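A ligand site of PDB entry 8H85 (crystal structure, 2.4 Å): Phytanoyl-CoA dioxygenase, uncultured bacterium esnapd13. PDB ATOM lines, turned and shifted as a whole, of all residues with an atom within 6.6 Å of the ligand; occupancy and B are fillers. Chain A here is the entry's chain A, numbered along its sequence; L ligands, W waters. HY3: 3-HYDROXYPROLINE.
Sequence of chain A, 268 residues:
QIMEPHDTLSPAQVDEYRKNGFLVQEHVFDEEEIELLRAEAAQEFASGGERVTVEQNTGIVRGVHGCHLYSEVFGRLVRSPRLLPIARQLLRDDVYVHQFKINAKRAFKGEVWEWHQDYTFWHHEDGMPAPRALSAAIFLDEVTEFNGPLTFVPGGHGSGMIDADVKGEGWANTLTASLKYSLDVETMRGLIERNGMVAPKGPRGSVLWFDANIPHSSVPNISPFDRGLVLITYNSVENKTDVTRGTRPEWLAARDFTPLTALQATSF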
ATOM      1  N   HIS A  65       8.174   5.575 -35.051  1.00  0.00           N
ATOM      2  CA  HIS A  65       8.397   7.009 -35.071  1.00  0.00           C
ATOM      3  C   HIS A  65       8.102   7.612 -36.460  1.00  0.00           C
ATOM      4  O   HIS A  65       8.438   7.010 -37.470  1.00  0.00           O
ATOM      5  CB  HIS A  65       9.842   7.289 -34.656  1.00  0.00           C
ATOM      6  CG  HIS A  65      10.083   7.133 -33.196  1.00  0.00           C
ATOM      7  ND1 HIS A  65      10.225   5.930 -32.574  1.00  0.00           N
ATOM      8  CD2 HIS A  65      10.206   8.119 -32.240  1.00  0.00           C
ATOM      9  CE1 HIS A  65      10.411   6.136 -31.275  1.00  0.00           C
ATOM     10  NE2 HIS A  65      10.428   7.506 -31.037  1.00  0.00           N
ATOM     11  N   HIS A  98       6.429  18.225 -33.981  1.00  0.00           N
ATOM     12  CA  HIS A  98       7.857  17.959 -33.871  1.00  0.00           C
ATOM     13  C   HIS A  98       8.168  16.461 -33.961  1.00  0.00           C
ATOM     14  O   HIS A  98       9.099  16.037 -34.650  1.00  0.00           O
ATOM     15  CB  HIS A  98       8.330  18.540 -32.538  1.00  0.00           C
ATOM     16  CG  HIS A  98       9.746  18.190 -32.208  1.00  0.00           C
ATOM     17  ND1 HIS A  98      10.810  18.559 -32.985  1.00  0.00           N
ATOM     18  CD2 HIS A  98      10.221  17.452 -31.160  1.00  0.00           C
ATOM     19  CE1 HIS A  98      11.923  18.057 -32.444  1.00  0.00           C
ATOM     20  NE2 HIS A  98      11.596  17.389 -31.280  1.00  0.00           N
ATOM     21  N   GLN A  99       7.336  15.640 -33.317  1.00  0.00           N
ATOM     22  CA  GLN A  99       7.623  14.223 -33.245  1.00  0.00           C
ATOM     23  C   GLN A  99       6.308  13.467 -33.119  1.00  0.00           C
ATOM     24  O   GLN A  99       5.398  13.916 -32.442  1.00  0.00           O
ATOM     25  CB  GLN A  99       8.559  13.979 -32.044  1.00  0.00           C
ATOM     26  CG  GLN A  99       8.897  12.527 -31.780  1.00  0.00           C
ATOM     27  CD  GLN A  99       9.928  12.363 -30.676  1.00  0.00           C
ATOM     28  OE1 GLN A  99       9.557  12.167 -29.524  1.00  0.00           O
ATOM     29  NE2 GLN A  99      11.219  12.440 -31.022  1.00  0.00           N
ATOM     30  N   LYS A 101       5.069   9.333 -32.291  1.00  0.00           N
ATOM     31  CA  LYS A 101       5.472   7.961 -32.037  1.00  0.00           C
ATOM     32  C   LYS A 101       4.321   7.159 -31.455  1.00  0.00           C
ATOM     33  O   LYS A 101       3.434   7.709 -30.767  1.00  0.00           O
ATOM     34  CB  LYS A 101       6.695   7.942 -31.108  1.00  0.00           C
ATOM     35  CG  LYS A 101       6.490   8.587 -29.758  1.00  0.00           C
ATOM     36  CD  LYS A 101       7.783   8.784 -28.955  1.00  0.00           C
ATOM     37  CE  LYS A 101       7.672   9.687 -27.726  1.00  0.00           C
ATOM     38  NZ  LYS A 101       7.503  11.136 -28.048  1.00  0.00           N
ATOM     39  N   TRP A 113      11.186   2.526 -17.908  1.00  0.00           N
ATOM     40  CA  TRP A 113      11.671   3.779 -18.452  1.00  0.00           C
ATOM     41  C   TRP A 113      12.134   4.688 -17.327  1.00  0.00           C
ATOM     42  O   TRP A 113      11.282   5.252 -16.636  1.00  0.00           O
ATOM     43  CB  TRP A 113      10.566   4.486 -19.254  1.00  0.00           C
ATOM     44  CG  TRP A 113      10.326   3.884 -20.595  1.00  0.00           C
ATOM     45  CD1 TRP A 113       9.811   2.652 -20.888  1.00  0.00           C
ATOM     46  CD2 TRP A 113      10.627   4.517 -21.848  1.00  0.00           C
ATOM     47  NE1 TRP A 113       9.745   2.485 -22.238  1.00  0.00           N
ATOM     48  CE2 TRP A 113      10.234   3.615 -22.863  1.00  0.00           C
ATOM     49  CE3 TRP A 113      11.158   5.762 -22.213  1.00  0.00           C
ATOM     50  CZ2 TRP A 113      10.367   3.925 -24.219  1.00  0.00           C
ATOM     51  CZ3 TRP A 113      11.281   6.065 -23.557  1.00  0.00           C
ATOM     52  CH2 TRP A 113      10.897   5.155 -24.545  1.00  0.00           C
ATOM     53  N   HIS A 116      13.028  10.986 -16.919  1.00  0.00           N
ATOM     54  CA  HIS A 116      13.561  11.890 -17.931  1.00  0.00           C
ATOM     55  C   HIS A 116      12.597  13.040 -18.214  1.00  0.00           C
ATOM     56  O   HIS A 116      11.419  12.997 -17.830  1.00  0.00           O
ATOM     57  CB  HIS A 116      13.849  11.194 -19.258  1.00  0.00           C
ATOM     58  CG  HIS A 116      12.639  10.532 -19.853  1.00  0.00           C
ATOM     59  ND1 HIS A 116      12.014   9.430 -19.283  1.00  0.00           N
ATOM     60  CD2 HIS A 116      11.960  10.852 -20.997  1.00  0.00           C
ATOM     61  CE1 HIS A 116      10.986   9.085 -20.065  1.00  0.00           C
ATOM     62  NE2 HIS A 116      10.926   9.963 -21.136  1.00  0.00           N
ATOM     63  N   GLN A 117      13.161  14.068 -18.850  1.00  0.00           N
ATOM     64  CA  GLN A 117      12.437  15.204 -19.415  1.00  0.00           C
ATOM     65  C   GLN A 117      12.622  15.194 -20.936  1.00  0.00           C
ATOM     66  O   GLN A 117      13.761  15.253 -21.368  1.00  0.00           O
ATOM     67  CB  GLN A 117      12.984  16.523 -18.878  1.00  0.00           C
ATOM     68  CG  GLN A 117      12.592  16.746 -17.434  1.00  0.00           C
ATOM     69  CD  GLN A 117      13.452  17.798 -16.773  1.00  0.00           C
ATOM     70  OE1 GLN A 117      14.681  17.656 -16.725  1.00  0.00           O
ATOM     71  NE2 GLN A 117      12.819  18.816 -16.221  1.00  0.00           N
ATOM     72  N   ASP A 118      11.516  15.128 -21.709  1.00  0.00           N
ATOM     73  CA  ASP A 118      11.561  15.230 -23.161  1.00  0.00           C
ATOM     74  C   ASP A 118      12.357  16.433 -23.650  1.00  0.00           C
ATOM     75  O   ASP A 118      13.118  16.284 -24.584  1.00  0.00           O
ATOM     76  CB  ASP A 118      10.155  15.363 -23.755  1.00  0.00           C
ATOM     77  CG  ASP A 118       9.329  14.082 -23.640  1.00  0.00           C
ATOM     78  OD1 ASP A 118       9.957  13.015 -23.471  1.00  0.00           O
ATOM     79  OD2 ASP A 118       8.053  14.187 -23.617  1.00  0.00           O
ATOM     80  N   PHE A 121      16.198  16.100 -24.275  1.00  0.00           N
ATOM     81  CA  PHE A 121      16.527  15.492 -25.569  1.00  0.00           C
ATOM     82  C   PHE A 121      16.288  16.483 -26.700  1.00  0.00           C
ATOM     83  O   PHE A 121      17.102  16.569 -27.617  1.00  0.00           O
ATOM     84  CB  PHE A 121      15.686  14.246 -25.876  1.00  0.00           C
ATOM     85  CG  PHE A 121      15.862  13.078 -24.950  1.00  0.00           C
ATOM     86  CD1 PHE A 121      15.361  13.098 -23.648  1.00  0.00           C
ATOM     87  CD2 PHE A 121      16.506  11.926 -25.380  1.00  0.00           C
ATOM     88  CE1 PHE A 121      15.527  12.011 -22.782  1.00  0.00           C
ATOM     89  CE2 PHE A 121      16.672  10.839 -24.515  1.00  0.00           C
ATOM     90  CZ  PHE A 121      16.175  10.881 -23.230  1.00  0.00           C
ATOM     91  N   TRP A 122      15.182  17.224 -26.692  1.00  0.00           N
ATOM     92  CA  TRP A 122      14.848  18.029 -27.857  1.00  0.00           C
ATOM     93  C   TRP A 122      15.750  19.259 -27.913  1.00  0.00           C
ATOM     94  O   TRP A 122      16.113  19.700 -29.002  1.00  0.00           O
ATOM     95  CB  TRP A 122      13.353  18.399 -27.892  1.00  0.00           C
ATOM     96  CG  TRP A 122      12.450  17.190 -27.938  1.00  0.00           C
ATOM     97  CD1 TRP A 122      12.725  16.006 -28.549  1.00  0.00           C
ATOM     98  CD2 TRP A 122      11.098  17.078 -27.449  1.00  0.00           C
ATOM     99  NE1 TRP A 122      11.670  15.152 -28.419  1.00  0.00           N
ATOM    100  CE2 TRP A 122      10.666  15.774 -27.747  1.00  0.00           C
ATOM    101  CE3 TRP A 122      10.228  17.908 -26.740  1.00  0.00           C
ATOM    102  CZ2 TRP A 122       9.406  15.291 -27.386  1.00  0.00           C
ATOM    103  CZ3 TRP A 122       8.959  17.457 -26.410  1.00  0.00           C
ATOM    104  CH2 TRP A 122       8.571  16.150 -26.713  1.00  0.00           C
ATOM    105  N   GLU A 125      19.467  17.410 -28.783  1.00  0.00           N
ATOM    106  CA  GLU A 125      19.544  16.632 -30.019  1.00  0.00           C
ATOM    107  C   GLU A 125      19.059  17.460 -31.213  1.00  0.00           C
ATOM    108  O   GLU A 125      19.595  17.295 -32.306  1.00  0.00           O
ATOM    109  CB  GLU A 125      18.706  15.352 -29.954  1.00  0.00           C
ATOM    110  CG  GLU A 125      19.132  14.381 -28.869  1.00  0.00           C
ATOM    111  CD  GLU A 125      20.538  13.836 -29.019  1.00  0.00           C
ATOM    112  OE1 GLU A 125      20.850  13.255 -30.103  1.00  0.00           O
ATOM    113  OE2 GLU A 125      21.337  13.999 -28.070  1.00  0.00           O
ATOM    114  N   ASP A 126      18.027  18.317 -31.033  1.00  0.00           N
ATOM    115  CA  ASP A 126      17.283  18.850 -32.171  1.00  0.00           C
ATOM    116  C   ASP A 126      17.339  20.377 -32.251  1.00  0.00           C
ATOM    117  O   ASP A 126      16.950  20.911 -33.278  1.00  0.00           O
ATOM    118  CB  ASP A 126      15.817  18.416 -32.153  1.00  0.00           C
ATOM    119  CG  ASP A 126      15.604  16.914 -32.090  1.00  0.00           C
ATOM    120  OD1 ASP A 126      16.352  16.188 -32.760  1.00  0.00           O
ATOM    121  OD2 ASP A 126      14.667  16.502 -31.412  1.00  0.00           O
ATOM    122  N   SER A 135       3.110  17.030 -25.417  1.00  0.00           N
ATOM    123  CA  SER A 135       2.742  15.775 -26.040  1.00  0.00           C
ATOM    124  C   SER A 135       1.284  15.481 -25.689  1.00  0.00           C
ATOM    125  O   SER A 135       0.797  15.840 -24.611  1.00  0.00           O
ATOM    126  CB  SER A 135       3.721  14.703 -25.685  1.00  0.00           C
ATOM    127  OG  SER A 135       5.039  15.025 -26.200  1.00  0.00           O
ATOM    128  N   ASN A 173      20.775   5.969 -28.041  1.00  0.00           N
ATOM    129  CA  ASN A 173      19.748   5.551 -27.084  1.00  0.00           C
ATOM    130  C   ASN A 173      18.810   6.710 -26.727  1.00  0.00           C
ATOM    131  O   ASN A 173      18.786   7.209 -25.600  1.00  0.00           O
ATOM    132  CB  ASN A 173      20.354   4.813 -25.871  1.00  0.00           C
ATOM    133  CG  ASN A 173      21.719   5.301 -25.424  1.00  0.00           C
ATOM    134  OD1 ASN A 173      21.890   5.742 -24.292  1.00  0.00           O
ATOM    135  ND2 ASN A 173      22.712   5.171 -26.288  1.00  0.00           N
ATOM    136  N   THR A 174      17.981   7.128 -27.705  1.00  0.00           N
ATOM    137  CA  THR A 174      16.919   8.108 -27.523  1.00  0.00           C
ATOM    138  C   THR A 174      15.545   7.398 -27.518  1.00  0.00           C
ATOM    139  O   THR A 174      14.599   7.871 -26.887  1.00  0.00           O
ATOM    140  CB  THR A 174      17.042   9.270 -28.541  1.00  0.00           C
ATOM    141  OG1 THR A 174      17.083   8.828 -29.898  1.00  0.00           O
ATOM    142  CG2 THR A 174      18.263  10.131 -28.298  1.00  0.00           C
ATOM    143  N   LEU A 175      15.447   6.256 -28.199  1.00  0.00           N
ATOM    144  CA  LEU A 175      14.188   5.571 -28.465  1.00  0.00           C
ATOM    145  C   LEU A 175      13.993   4.409 -27.489  1.00  0.00           C
ATOM    146  O   LEU A 175      12.908   3.816 -27.459  1.00  0.00           O
ATOM    147  CB  LEU A 175      14.231   5.054 -29.910  1.00  0.00           C
ATOM    148  CG  LEU A 175      14.833   6.002 -30.955  1.00  0.00           C
ATOM    149  CD1 LEU A 175      14.861   5.361 -32.342  1.00  0.00           C
ATOM    150  CD2 LEU A 175      14.070   7.311 -30.964  1.00  0.00           C
ATOM    151  N   THR A 176      15.039   4.089 -26.709  1.00  0.00           N
ATOM    152  CA  THR A 176      15.116   2.884 -25.891  1.00  0.00           C
ATOM    153  C   THR A 176      15.071   3.246 -24.403  1.00  0.00           C
ATOM    154  O   THR A 176      15.452   4.351 -24.014  1.00  0.00           O
ATOM    155  CB  THR A 176      16.364   2.069 -26.285  1.00  0.00           C
ATOM    156  OG1 THR A 176      17.536   2.843 -26.040  1.00  0.00           O
ATOM    157  CG2 THR A 176      16.358   1.653 -27.739  1.00  0.00           C
ATOM    158  N   LEU A 179      18.123   5.280 -21.253  1.00  0.00           N
ATOM    159  CA  LEU A 179      18.062   6.588 -21.903  1.00  0.00           C
ATOM    160  C   LEU A 179      19.378   7.369 -21.781  1.00  0.00           C
ATOM    161  O   LEU A 179      20.097   7.318 -20.779  1.00  0.00           O
ATOM    162  CB  LEU A 179      16.889   7.389 -21.320  1.00  0.00           C
ATOM    163  CG  LEU A 179      15.485   6.930 -21.702  1.00  0.00           C
ATOM    164  CD1 LEU A 179      14.436   7.682 -20.890  1.00  0.00           C
ATOM    165  CD2 LEU A 179      15.218   7.117 -23.199  1.00  0.00           C
ATOM    166  N   HIS A 216       9.089  12.273 -16.248  1.00  0.00           N
ATOM    167  CA  HIS A 216       8.181  11.136 -16.282  1.00  0.00           C
ATOM    168  C   HIS A 216       8.938   9.834 -16.444  1.00  0.00           C
ATOM    169  O   HIS A 216      10.081   9.791 -16.929  1.00  0.00           O
ATOM    170  CB  HIS A 216       7.153  11.277 -17.405  1.00  0.00           C
ATOM    171  CG  HIS A 216       7.686  11.293 -18.806  1.00  0.00           C
ATOM    172  ND1 HIS A 216       8.182  12.405 -19.395  1.00  0.00           N
ATOM    173  CD2 HIS A 216       7.688  10.339 -19.772  1.00  0.00           C
ATOM    174  CE1 HIS A 216       8.562  12.137 -20.640  1.00  0.00           C
ATOM    175  NE2 HIS A 216       8.235  10.883 -20.904  1.00  0.00           N
ATOM    176  N   THR A 233       3.762  15.040 -30.416  1.00  0.00           N
ATOM    177  CA  THR A 233       4.418  16.158 -29.787  1.00  0.00           C
ATOM    178  C   THR A 233       4.201  17.403 -30.656  1.00  0.00           C
ATOM    179  O   THR A 233       4.695  17.466 -31.789  1.00  0.00           O
ATOM    180  CB  THR A 233       5.896  15.885 -29.544  1.00  0.00           C
ATOM    181  OG1 THR A 233       6.074  14.797 -28.628  1.00  0.00           O
ATOM    182  CG2 THR A 233       6.542  17.115 -28.935  1.00  0.00           C
ATOM    183  N   ARG A 248      19.227  14.625 -35.943  1.00  0.00           N
ATOM    184  CA  ARG A 248      18.394  13.443 -36.104  1.00  0.00           C
ATOM    185  C   ARG A 248      17.541  13.550 -37.361  1.00  0.00           C
ATOM    186  O   ARG A 248      17.334  14.641 -37.862  1.00  0.00           O
ATOM    187  CB  ARG A 248      17.507  13.257 -34.874  1.00  0.00           C
ATOM    188  CG  ARG A 248      18.281  13.250 -33.561  1.00  0.00           C
ATOM    189  CD  ARG A 248      17.499  12.603 -32.457  1.00  0.00           C
ATOM    190  NE  ARG A 248      16.301  13.328 -32.040  1.00  0.00           N
ATOM    191  CZ  ARG A 248      15.522  12.944 -31.024  1.00  0.00           C
ATOM    192  NH1 ARG A 248      15.580  11.699 -30.551  1.00  0.00           N
ATOM    193  NH2 ARG A 248      14.693  13.810 -30.472  1.00  0.00           N
ATOM    194  N   LEU A 252      12.233  11.630 -36.479  1.00  0.00           N
ATOM    195  CA  LEU A 252      12.396  11.872 -35.042  1.00  0.00           C
ATOM    196  C   LEU A 252      12.176  13.349 -34.671  1.00  0.00           C
ATOM    197  O   LEU A 252      11.813  13.652 -33.531  1.00  0.00           O
ATOM    198  CB  LEU A 252      13.787  11.423 -34.601  1.00  0.00           C
ATOM    199  CG  LEU A 252      14.080   9.923 -34.675  1.00  0.00           C
ATOM    200  CD1 LEU A 252      15.465   9.631 -34.121  1.00  0.00           C
ATOM    201  CD2 LEU A 252      13.022   9.120 -33.905  1.00  0.00           C
HETATM  202  C   HY3 L   1      13.170  11.473 -27.977  1.00  0.00           C
HETATM  203  O   HY3 L   1      12.986  12.478 -28.587  1.00  0.00           O
HETATM  204  N   HY3 L   1      12.133   9.428 -26.787  1.00  0.00           N
HETATM  205  CA  HY3 L   1      11.955  10.817 -27.287  1.00  0.00           C
HETATM  206  C3  HY3 L   1      11.607  11.626 -26.027  1.00  0.00           C
HETATM  207  C4  HY3 L   1      12.346  10.899 -24.911  1.00  0.00           C
HETATM  208  C5  HY3 L   1      12.336   9.435 -25.332  1.00  0.00           C
HETATM  209  O2  HY3 L   1      10.186  11.632 -25.886  1.00  0.00           O
HETATM  210  OXT HY3 L   1      14.233  10.953 -27.818  1.00  0.00           O
HETATM  211  O   HOH W   1       6.876  12.601 -25.726  1.00  0.00           O
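OD1 of Asp 118 is in hydrogen-bond range of O2 of the ligand, at 2.8 Å. The indole nitrogen (NE1) of Trp 122 lies within hydrogen-bond range of an oxygen (O) of the ligand (3.0 Å). An oxygen (O) of the ligand sits at hydrogen-bond distance from the side-chain amide nitrogen (NE2) of Gln 99 (3.0 Å). The backbone carbonyl oxygen (O) of Thr 174 is in hydrogen-bond range of a nitrogen (N) of the ligand (2.9 Å). O of the ligand lies within salt-bridge range of NH2 of Arg 248 (2.9 Å). NZ of Lys 101 sits at hydrogen-bond distance from O2 of the ligand (3.5 Å).
NE2 of Gln 99 sits at hydrogen-bond distance from O of Leu 252, at 2.8 Å. The side-chain amide oxygen of Gln 99 sits at hydrogen-bond distance from the side-chain amino group of Lys 101 (2.7 Å). O of Gln 99 is in hydrogen-bond range of N of Thr 233 (2.8 Å). NE2 of His 116 lies within hydrogen-bond range of NE2 of His 216 (2.9 Å). NH2 of Arg 248 is in salt-bridge range of OD2 of Asp 126 (2.9 Å). NH1 of Arg 248 sits at hydrogen-bond distance from OG1 of Thr 174, at 3.3 Å.
Trp 113 touches the ligand. CD2 of His 116 touches C4 of the ligand, 3.9 Å away. Phe 121 touches the ligand (CD2 to OXT, 3.5 Å). Hydrophobic or aromatic side chains within 4 Å of the ligand: Trp 113, His 116, Phe 121 and Trp 122. Within 4 Å of the ligand: Gln 99, Lys 101, Trp 113, His 116, Asp 118, Phe 121, Trp 122, Thr 174 and Arg 248.
Water W1 lies within hydrogen-bond range of the side-chain amino group (NZ) of Lys 101 (2.8 Å), the side-chain carboxylate (OD2) of Asp 118 (2.9 Å), the side-chain hydroxyl (OG) of Ser 135 (3.1 Å) and an oxygen (O2) of the ligand (3.5 Å).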
